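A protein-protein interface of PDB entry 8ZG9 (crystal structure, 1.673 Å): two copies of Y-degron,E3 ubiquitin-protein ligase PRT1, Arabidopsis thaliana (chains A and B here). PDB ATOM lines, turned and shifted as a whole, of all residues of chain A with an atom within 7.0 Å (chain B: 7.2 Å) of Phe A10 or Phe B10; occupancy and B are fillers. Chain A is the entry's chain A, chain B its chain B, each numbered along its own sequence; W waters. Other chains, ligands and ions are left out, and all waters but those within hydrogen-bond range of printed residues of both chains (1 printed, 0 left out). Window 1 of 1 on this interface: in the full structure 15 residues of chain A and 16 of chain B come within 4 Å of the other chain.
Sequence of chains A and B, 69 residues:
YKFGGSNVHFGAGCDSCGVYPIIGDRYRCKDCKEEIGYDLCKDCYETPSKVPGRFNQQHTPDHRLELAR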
ATOM      1  N   LYS A   2     -21.377  -1.732   4.853  1.00  0.00           N
ATOM      2  CA  LYS A   2     -21.597  -0.512   4.085  1.00  0.00           C
ATOM      3  C   LYS A   2     -22.964  -0.636   3.428  1.00  0.00           C
ATOM      4  O   LYS A   2     -23.132  -1.415   2.479  1.00  0.00           O
ATOM      5  CB  LYS A   2     -20.519  -0.317   3.030  1.00  0.00           C
ATOM      6  CG  LYS A   2     -20.494   1.089   2.448  1.00  0.00           C
ATOM      7  CD  LYS A   2     -21.655   1.164   1.470  1.00  0.00           C
ATOM      8  CE  LYS A   2     -21.624   2.340   0.553  1.00  0.00           C
ATOM      9  NZ  LYS A   2     -22.741   2.290  -0.408  1.00  0.00           N
ATOM     10  N   PHE A   3     -23.908   0.197   3.869  1.00  0.00           N
ATOM     11  CA  PHE A   3     -25.267   0.125   3.358  1.00  0.00           C
ATOM     12  C   PHE A   3     -25.321   0.534   1.891  1.00  0.00           C
ATOM     13  O   PHE A   3     -24.715   1.531   1.485  1.00  0.00           O
ATOM     14  CB  PHE A   3     -26.190   1.026   4.176  1.00  0.00           C
ATOM     15  CG  PHE A   3     -26.241   0.685   5.634  1.00  0.00           C
ATOM     16  CD1 PHE A   3     -26.722  -0.542   6.040  1.00  0.00           C
ATOM     17  CD2 PHE A   3     -25.849   1.594   6.596  1.00  0.00           C
ATOM     18  CE1 PHE A   3     -26.784  -0.871   7.372  1.00  0.00           C
ATOM     19  CE2 PHE A   3     -25.914   1.276   7.936  1.00  0.00           C
ATOM     20  CZ  PHE A   3     -26.379   0.040   8.327  1.00  0.00           C
ATOM     21  N   GLY A   4     -26.092  -0.222   1.106  1.00  0.00           N
ATOM     22  CA  GLY A   4     -26.242   0.044  -0.307  1.00  0.00           C
ATOM     23  C   GLY A   4     -25.162  -0.536  -1.194  1.00  0.00           C
ATOM     24  O   GLY A   4     -25.320  -0.518  -2.420  1.00  0.00           O
ATOM     25  N   GLY A   5     -24.054  -1.019  -0.633  1.00  0.00           N
ATOM     26  CA  GLY A   5     -23.072  -1.668  -1.486  1.00  0.00           C
ATOM     27  C   GLY A   5     -22.510  -0.696  -2.505  1.00  0.00           C
ATOM     28  O   GLY A   5     -22.250   0.479  -2.215  1.00  0.00           O
ATOM     29  N   VAL A   8     -24.621   2.866  -4.430  1.00  0.00           N
ATOM     30  CA  VAL A   8     -24.631   4.249  -3.966  1.00  0.00           C
ATOM     31  C   VAL A   8     -23.284   4.584  -3.349  1.00  0.00           C
ATOM     32  O   VAL A   8     -22.641   3.740  -2.717  1.00  0.00           O
ATOM     33  CB  VAL A   8     -25.796   4.483  -2.978  1.00  0.00           C
ATOM     34  CG1 VAL A   8     -25.538   3.770  -1.673  1.00  0.00           C
ATOM     35  CG2 VAL A   8     -25.978   5.972  -2.693  1.00  0.00           C
ATOM     36  N   HIS A   9     -22.846   5.825  -3.560  1.00  0.00           N
ATOM     37  CA  HIS A   9     -21.547   6.302  -3.097  1.00  0.00           C
ATOM     38  C   HIS A   9     -21.794   7.552  -2.275  1.00  0.00           C
ATOM     39  O   HIS A   9     -21.758   8.674  -2.787  1.00  0.00           O
ATOM     40  CB  HIS A   9     -20.675   6.503  -4.282  1.00  0.00           C
ATOM     41  CG  HIS A   9     -20.624   5.290  -5.155  1.00  0.00           C
ATOM     42  ND1 HIS A   9     -19.630   4.342  -5.051  1.00  0.00           N
ATOM     43  CD2 HIS A   9     -21.495   4.822  -6.082  1.00  0.00           C
ATOM     44  CE1 HIS A   9     -19.865   3.367  -5.913  1.00  0.00           C
ATOM     45  NE2 HIS A   9     -20.989   3.636  -6.552  1.00  0.00           N
ATOM     46  N   PHE A  10     -22.102   7.330  -0.998  1.00  0.00           N
ATOM     47  CA  PHE A  10     -22.359   8.438  -0.101  1.00  0.00           C
ATOM     48  C   PHE A  10     -21.106   9.305  -0.060  1.00  0.00           C
ATOM     49  O   PHE A  10     -19.977   8.800  -0.018  1.00  0.00           O
ATOM     50  CB  PHE A  10     -22.704   7.928   1.309  1.00  0.00           C
ATOM     51  CG  PHE A  10     -23.921   7.039   1.371  1.00  0.00           C
ATOM     52  CD1 PHE A  10     -25.157   7.492   0.956  1.00  0.00           C
ATOM     53  CD2 PHE A  10     -23.823   5.746   1.867  1.00  0.00           C
ATOM     54  CE1 PHE A  10     -26.270   6.671   1.015  1.00  0.00           C
ATOM     55  CE2 PHE A  10     -24.929   4.923   1.929  1.00  0.00           C
ATOM     56  CZ  PHE A  10     -26.154   5.388   1.512  1.00  0.00           C
ATOM     57  N   GLY A  11     -21.304  10.613  -0.084  1.00  0.00           N
ATOM     58  CA  GLY A  11     -20.200  11.546  -0.045  1.00  0.00           C
ATOM     59  C   GLY A  11     -19.479  11.790  -1.354  1.00  0.00           C
ATOM     60  O   GLY A  11     -18.544  12.599  -1.375  1.00  0.00           O
ATOM     61  N   ALA A  12     -19.868  11.132  -2.441  1.00  0.00           N
ATOM     62  CA  ALA A  12     -19.215  11.299  -3.731  1.00  0.00           C
ATOM     63  C   ALA A  12     -20.178  11.957  -4.706  1.00  0.00           C
ATOM     64  O   ALA A  12     -21.332  11.532  -4.825  1.00  0.00           O
ATOM     65  CB  ALA A  12     -18.740   9.955  -4.284  1.00  0.00           C
ATOM     66  N   GLY A  13     -19.701  12.993  -5.396  1.00  0.00           N
ATOM     67  CA  GLY A  13     -20.483  13.658  -6.416  1.00  0.00           C
ATOM     68  C   GLY A  13     -19.792  13.595  -7.759  1.00  0.00           C
ATOM     69  O   GLY A  13     -18.568  13.444  -7.824  1.00  0.00           O
ATOM     70  N   TYR A  20     -25.138  14.193  -6.744  1.00  0.00           N
ATOM     71  CA  TYR A  20     -24.615  13.834  -5.432  1.00  0.00           C
ATOM     72  C   TYR A  20     -25.751  13.404  -4.511  1.00  0.00           C
ATOM     73  O   TYR A  20     -26.737  14.142  -4.339  1.00  0.00           O
ATOM     74  CB  TYR A  20     -23.818  14.992  -4.851  1.00  0.00           C
ATOM     75  CG  TYR A  20     -23.299  14.778  -3.459  1.00  0.00           C
ATOM     76  CD1 TYR A  20     -24.159  14.614  -2.378  1.00  0.00           C
ATOM     77  CD2 TYR A  20     -21.939  14.713  -3.227  1.00  0.00           C
ATOM     78  CE1 TYR A  20     -23.666  14.433  -1.101  1.00  0.00           C
ATOM     79  CE2 TYR A  20     -21.440  14.510  -1.959  1.00  0.00           C
ATOM     80  CZ  TYR A  20     -22.309  14.380  -0.902  1.00  0.00           C
ATOM     81  OH  TYR A  20     -21.810  14.193   0.362  1.00  0.00           O
ATOM     82  N   PRO A  21     -25.657  12.209  -3.905  1.00  0.00           N
ATOM     83  CA  PRO A  21     -24.589  11.205  -4.076  1.00  0.00           C
ATOM     84  C   PRO A  21     -24.655  10.515  -5.441  1.00  0.00           C
ATOM     85  O   PRO A  21     -25.738  10.471  -6.011  1.00  0.00           O
ATOM     86  CB  PRO A  21     -24.878  10.198  -2.966  1.00  0.00           C
ATOM     87  CG  PRO A  21     -26.360  10.283  -2.803  1.00  0.00           C
ATOM     88  CD  PRO A  21     -26.683  11.747  -2.957  1.00  0.00           C
ATOM     89  N   ILE A  22     -23.547   9.981  -5.957  1.00  0.00           N
ATOM     90  CA  ILE A  22     -23.621   9.173  -7.168  1.00  0.00           C
ATOM     91  C   ILE A  22     -24.420   7.913  -6.870  1.00  0.00           C
ATOM     92  O   ILE A  22     -24.120   7.179  -5.919  1.00  0.00           O
ATOM     93  CB  ILE A  22     -22.213   8.837  -7.687  1.00  0.00           C
ATOM     94  CG1 ILE A  22     -21.503  10.110  -8.159  1.00  0.00           C
ATOM     95  CG2 ILE A  22     -22.297   7.811  -8.805  1.00  0.00           C
ATOM     96  CD1 ILE A  22     -20.032   9.923  -8.479  1.00  0.00           C
ATOM     97  N   ARG A  26     -19.774   4.156 -10.067  1.00  0.00           N
ATOM     98  CA  ARG A  26     -18.910   5.308  -9.859  1.00  0.00           C
ATOM     99  C   ARG A  26     -17.518   5.013 -10.419  1.00  0.00           C
ATOM    100  O   ARG A  26     -16.963   3.932 -10.187  1.00  0.00           O
ATOM    101  CB  ARG A  26     -18.792   5.638  -8.378  1.00  0.00           C
ATOM    102  CG  ARG A  26     -17.718   6.644  -8.030  1.00  0.00           C
ATOM    103  CD  ARG A  26     -17.463   6.690  -6.542  1.00  0.00           C
ATOM    104  NE  ARG A  26     -16.303   7.502  -6.193  1.00  0.00           N
ATOM    105  CZ  ARG A  26     -15.694   7.442  -5.017  1.00  0.00           C
ATOM    106  NH1 ARG A  26     -16.131   6.607  -4.087  1.00  0.00           N
ATOM    107  NH2 ARG A  26     -14.660   8.225  -4.763  1.00  0.00           N
ATOM    108  N   LYS B   2     -15.176  13.759  -3.591  1.00  0.00           N
ATOM    109  CA  LYS B   2     -15.590  13.002  -2.412  1.00  0.00           C
ATOM    110  C   LYS B   2     -15.162  13.812  -1.195  1.00  0.00           C
ATOM    111  O   LYS B   2     -13.960  13.899  -0.895  1.00  0.00           O
ATOM    112  CB  LYS B   2     -14.938  11.620  -2.367  1.00  0.00           C
ATOM    113  CG  LYS B   2     -15.601  10.664  -1.394  1.00  0.00           C
ATOM    114  CD  LYS B   2     -15.200  11.077   0.033  1.00  0.00           C
ATOM    115  CE  LYS B   2     -15.525  10.029   1.079  1.00  0.00           C
ATOM    116  NZ  LYS B   2     -15.057  10.396   2.422  1.00  0.00           N
ATOM    117  N   PHE B   3     -16.145  14.356  -0.465  1.00  0.00           N
ATOM    118  CA  PHE B   3     -15.855  15.181   0.703  1.00  0.00           C
ATOM    119  C   PHE B   3     -15.247  14.333   1.811  1.00  0.00           C
ATOM    120  O   PHE B   3     -15.709  13.224   2.094  1.00  0.00           O
ATOM    121  CB  PHE B   3     -17.116  15.890   1.209  1.00  0.00           C
ATOM    122  CG  PHE B   3     -17.740  16.781   0.179  1.00  0.00           C
ATOM    123  CD1 PHE B   3     -17.017  17.853  -0.327  1.00  0.00           C
ATOM    124  CD2 PHE B   3     -19.024  16.567  -0.286  1.00  0.00           C
ATOM    125  CE1 PHE B   3     -17.552  18.676  -1.298  1.00  0.00           C
ATOM    126  CE2 PHE B   3     -19.569  17.394  -1.254  1.00  0.00           C
ATOM    127  CZ  PHE B   3     -18.831  18.447  -1.761  1.00  0.00           C
ATOM    128  N   GLY B   4     -14.209  14.877   2.445  1.00  0.00           N
ATOM    129  CA  GLY B   4     -13.525  14.186   3.515  1.00  0.00           C
ATOM    130  C   GLY B   4     -12.460  13.212   3.069  1.00  0.00           C
ATOM    131  O   GLY B   4     -11.715  12.706   3.922  1.00  0.00           O
ATOM    132  N   GLY B   5     -12.380  12.896   1.779  1.00  0.00           N
ATOM    133  CA  GLY B   5     -11.308  12.022   1.350  1.00  0.00           C
ATOM    134  C   GLY B   5     -11.431  10.686   2.043  1.00  0.00           C
ATOM    135  O   GLY B   5     -12.527  10.159   2.274  1.00  0.00           O
ATOM    136  N   VAL B   8     -13.026   9.753   6.165  1.00  0.00           N
ATOM    137  CA  VAL B   8     -14.390   9.358   6.508  1.00  0.00           C
ATOM    138  C   VAL B   8     -14.973   8.481   5.406  1.00  0.00           C
ATOM    139  O   VAL B   8     -14.710   8.699   4.217  1.00  0.00           O
ATOM    140  CB  VAL B   8     -15.262  10.601   6.780  1.00  0.00           C
ATOM    141  CG1 VAL B   8     -15.633  11.285   5.502  1.00  0.00           C
ATOM    142  CG2 VAL B   8     -16.541  10.219   7.504  1.00  0.00           C
ATOM    143  N   HIS B   9     -15.751   7.472   5.826  1.00  0.00           N
ATOM    144  CA  HIS B   9     -16.379   6.487   4.943  1.00  0.00           C
ATOM    145  C   HIS B   9     -17.870   6.491   5.253  1.00  0.00           C
ATOM    146  O   HIS B   9     -18.361   5.700   6.061  1.00  0.00           O
ATOM    147  CB  HIS B   9     -15.706   5.160   5.143  1.00  0.00           C
ATOM    148  CG  HIS B   9     -14.218   5.264   5.039  1.00  0.00           C
ATOM    149  ND1 HIS B   9     -13.544   5.048   3.860  1.00  0.00           N
ATOM    150  CD2 HIS B   9     -13.284   5.637   5.947  1.00  0.00           C
ATOM    151  CE1 HIS B   9     -12.253   5.248   4.051  1.00  0.00           C
ATOM    152  NE2 HIS B   9     -12.069   5.606   5.310  1.00  0.00           N
ATOM    153  N   PHE B  10     -18.576   7.419   4.611  1.00  0.00           N
ATOM    154  CA  PHE B  10     -19.998   7.585   4.856  1.00  0.00           C
ATOM    155  C   PHE B  10     -20.732   6.294   4.520  1.00  0.00           C
ATOM    156  O   PHE B  10     -20.455   5.648   3.504  1.00  0.00           O
ATOM    157  CB  PHE B  10     -20.552   8.734   4.009  1.00  0.00           C
ATOM    158  CG  PHE B  10     -19.927  10.071   4.291  1.00  0.00           C
ATOM    159  CD1 PHE B  10     -19.998  10.634   5.547  1.00  0.00           C
ATOM    160  CD2 PHE B  10     -19.285  10.770   3.283  1.00  0.00           C
ATOM    161  CE1 PHE B  10     -19.427  11.869   5.804  1.00  0.00           C
ATOM    162  CE2 PHE B  10     -18.707  12.002   3.532  1.00  0.00           C
ATOM    163  CZ  PHE B  10     -18.788  12.558   4.793  1.00  0.00           C
ATOM    164  N   GLY B  11     -21.677   5.925   5.376  1.00  0.00           N
ATOM    165  CA  GLY B  11     -22.431   4.711   5.171  1.00  0.00           C
ATOM    166  C   GLY B  11     -21.726   3.437   5.575  1.00  0.00           C
ATOM    167  O   GLY B  11     -22.305   2.355   5.413  1.00  0.00           O
ATOM    168  N   ALA B  12     -20.501   3.518   6.082  1.00  0.00           N
ATOM    169  CA  ALA B  12     -19.725   2.347   6.458  1.00  0.00           C
ATOM    170  C   ALA B  12     -19.570   2.315   7.968  1.00  0.00           C
ATOM    171  O   ALA B  12     -19.191   3.319   8.582  1.00  0.00           O
ATOM    172  CB  ALA B  12     -18.348   2.361   5.795  1.00  0.00           C
ATOM    173  N   GLY B  13     -19.866   1.165   8.559  1.00  0.00           N
ATOM    174  CA  GLY B  13     -19.682   0.980   9.980  1.00  0.00           C
ATOM    175  C   GLY B  13     -18.723  -0.152  10.264  1.00  0.00           C
ATOM    176  O   GLY B  13     -18.542  -1.055   9.439  1.00  0.00           O
ATOM    177  N   TYR B  20     -19.740   4.428  13.410  1.00  0.00           N
ATOM    178  CA  TYR B  20     -20.406   4.734  12.148  1.00  0.00           C
ATOM    179  C   TYR B  20     -20.661   6.234  12.021  1.00  0.00           C
ATOM    180  O   TYR B  20     -21.298   6.827  12.900  1.00  0.00           O
ATOM    181  CB  TYR B  20     -21.712   3.943  12.067  1.00  0.00           C
ATOM    182  CG  TYR B  20     -22.548   4.210  10.840  1.00  0.00           C
ATOM    183  CD1 TYR B  20     -23.376   5.320  10.772  1.00  0.00           C
ATOM    184  CD2 TYR B  20     -22.505   3.352   9.749  1.00  0.00           C
ATOM    185  CE1 TYR B  20     -24.154   5.566   9.653  1.00  0.00           C
ATOM    186  CE2 TYR B  20     -23.269   3.599   8.621  1.00  0.00           C
ATOM    187  CZ  TYR B  20     -24.090   4.705   8.586  1.00  0.00           C
ATOM    188  OH  TYR B  20     -24.845   4.946   7.469  1.00  0.00           O
ATOM    189  N   PRO B  21     -20.164   6.896  10.967  1.00  0.00           N
ATOM    190  CA  PRO B  21     -19.300   6.332   9.917  1.00  0.00           C
ATOM    191  C   PRO B  21     -17.901   6.023  10.426  1.00  0.00           C
ATOM    192  O   PRO B  21     -17.475   6.639  11.398  1.00  0.00           O
ATOM    193  CB  PRO B  21     -19.258   7.438   8.859  1.00  0.00           C
ATOM    194  CG  PRO B  21     -19.427   8.694   9.641  1.00  0.00           C
ATOM    195  CD  PRO B  21     -20.436   8.328  10.740  1.00  0.00           C
ATOM    196  N   ILE B  22     -17.190   5.095   9.781  1.00  0.00           N
ATOM    197  CA  ILE B  22     -15.790   4.880  10.125  1.00  0.00           C
ATOM    198  C   ILE B  22     -15.006   6.138   9.784  1.00  0.00           C
ATOM    199  O   ILE B  22     -15.082   6.649   8.660  1.00  0.00           O
ATOM    200  CB  ILE B  22     -15.225   3.654   9.384  1.00  0.00           C
ATOM    201  CG1 ILE B  22     -15.873   2.358   9.885  1.00  0.00           C
ATOM    202  CG2 ILE B  22     -13.703   3.602   9.519  1.00  0.00           C
ATOM    203  CD1 ILE B  22     -15.532   1.143   9.052  1.00  0.00           C
ATOM    204  N   ARG B  26     -10.005   2.686   6.694  1.00  0.00           N
ATOM    205  CA  ARG B  26     -11.061   1.687   6.625  1.00  0.00           C
ATOM    206  C   ARG B  26     -10.495   0.417   6.006  1.00  0.00           C
ATOM    207  O   ARG B  26      -9.756   0.474   5.013  1.00  0.00           O
ATOM    208  CB  ARG B  26     -12.226   2.184   5.783  1.00  0.00           C
ATOM    209  CG  ARG B  26     -13.269   1.121   5.416  1.00  0.00           C
ATOM    210  CD  ARG B  26     -14.267   1.640   4.402  1.00  0.00           C
ATOM    211  NE  ARG B  26     -15.149   0.581   3.933  1.00  0.00           N
ATOM    212  CZ  ARG B  26     -15.910   0.672   2.852  1.00  0.00           C
ATOM    213  NH1 ARG B  26     -15.908   1.777   2.118  1.00  0.00           N
ATOM    214  NH2 ARG B  26     -16.688  -0.341   2.514  1.00  0.00           N
HETATM  215  O   HOH W   1     -17.304   8.039   1.932  1.00  0.00           O
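Water W1 lies within hydrogen-bond range of the backbone NH of Phe B10 (3.0 Å), the side-chain amino group of Lys B2 (3.3 Å) and the backbone carbonyl oxygen of Phe A10 (3.4 Å).
The side-chain amino group of Lys A2 is in hydrogen-bond range of the backbone carbonyl oxygen of Gly A5, at 2.6 Å. The backbone carbonyl oxygen (O) of Val A8 lies within hydrogen-bond range of the side-chain amino group (NZ) of Lys A2, at 2.7 Å. NZ of Lys B2 sits at hydrogen-bond distance from O of Gly B5 (2.5 Å). The backbone carbonyl oxygen of Val B8 sits at hydrogen-bond distance from the side-chain amino group of Lys B2, 2.5 Å away.
His A9 touches none of the printed residues of chain B. Of chain B, only Phe B10 (3.5 Å) and Gly B11 (3.7 Å) come within 4 Å of Phe A10. Of the printed residues of chain B, Tyr A20 touches Phe B3. Of chain A, only Phe A10 (3.5 Å) and Gly A11 (3.5 Å) come within 4 Å of Phe B10. Of the printed residues of chain A, Gly B11 touches Lys A2, Phe A3 and Phe A10. The nearest residue of chain B that does not touch Phe A10 is Lys B2 (4.7 Å). The nearest residue of chain A that does not touch Phe B10 is Lys A2 (4.6 Å).
Among the printed residues, pairs that only touch across the chains: Lys A2 with Gly B11, Lys A2 with Arg B26, Phe A3 with Tyr B20, Phe A10 with Phe B10, Phe A10 with Gly B11, Gly A11 with Lys B2, Gly A11 with Phe B10 and Tyr A20 with Phe B3.
The backbone NH (N) of Phe A3 lies within hydrogen-bond range of the backbone carbonyl oxygen (O) of Gly B11 (3.1 Å). N of Phe B3 is in hydrogen-bond range of O of Gly A11 (3.1 Å).
Lys A2 touches Gly B11, and with the chains exchanged Gly A11 touches Lys B2. Lys A2 touches Arg B26, but with the chains exchanged Arg A26 does not touch Lys B2 (4.2 Å). Phe A3 touches Gly B11, and with the chains exchanged Gly A11 touches Phe B3. Phe A10 touches Gly B11, and with the chains exchanged Gly A11 touches Phe B10. Of the 10 pairs that touch across the chains among the printed residues, 9 have their exchanged pair printed and touching as well.
Along chain A the printed residues that touch a printed residue of chain B span positions 2 to 20. Of the 14 printed residues of chain B, 6 touch a printed residue of chain A. Hydrophobic or aromatic side chains of chain B within 4 Å of the printed part of chain A: Phe B3, Phe B10 and Tyr B20. Among the printed residues, 10 pairs touch across the chains. Among the printed residues, no Asp or Glu carboxylate lies within 4 Å of a Lys or Arg side-chain nitrogen of the other chain.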
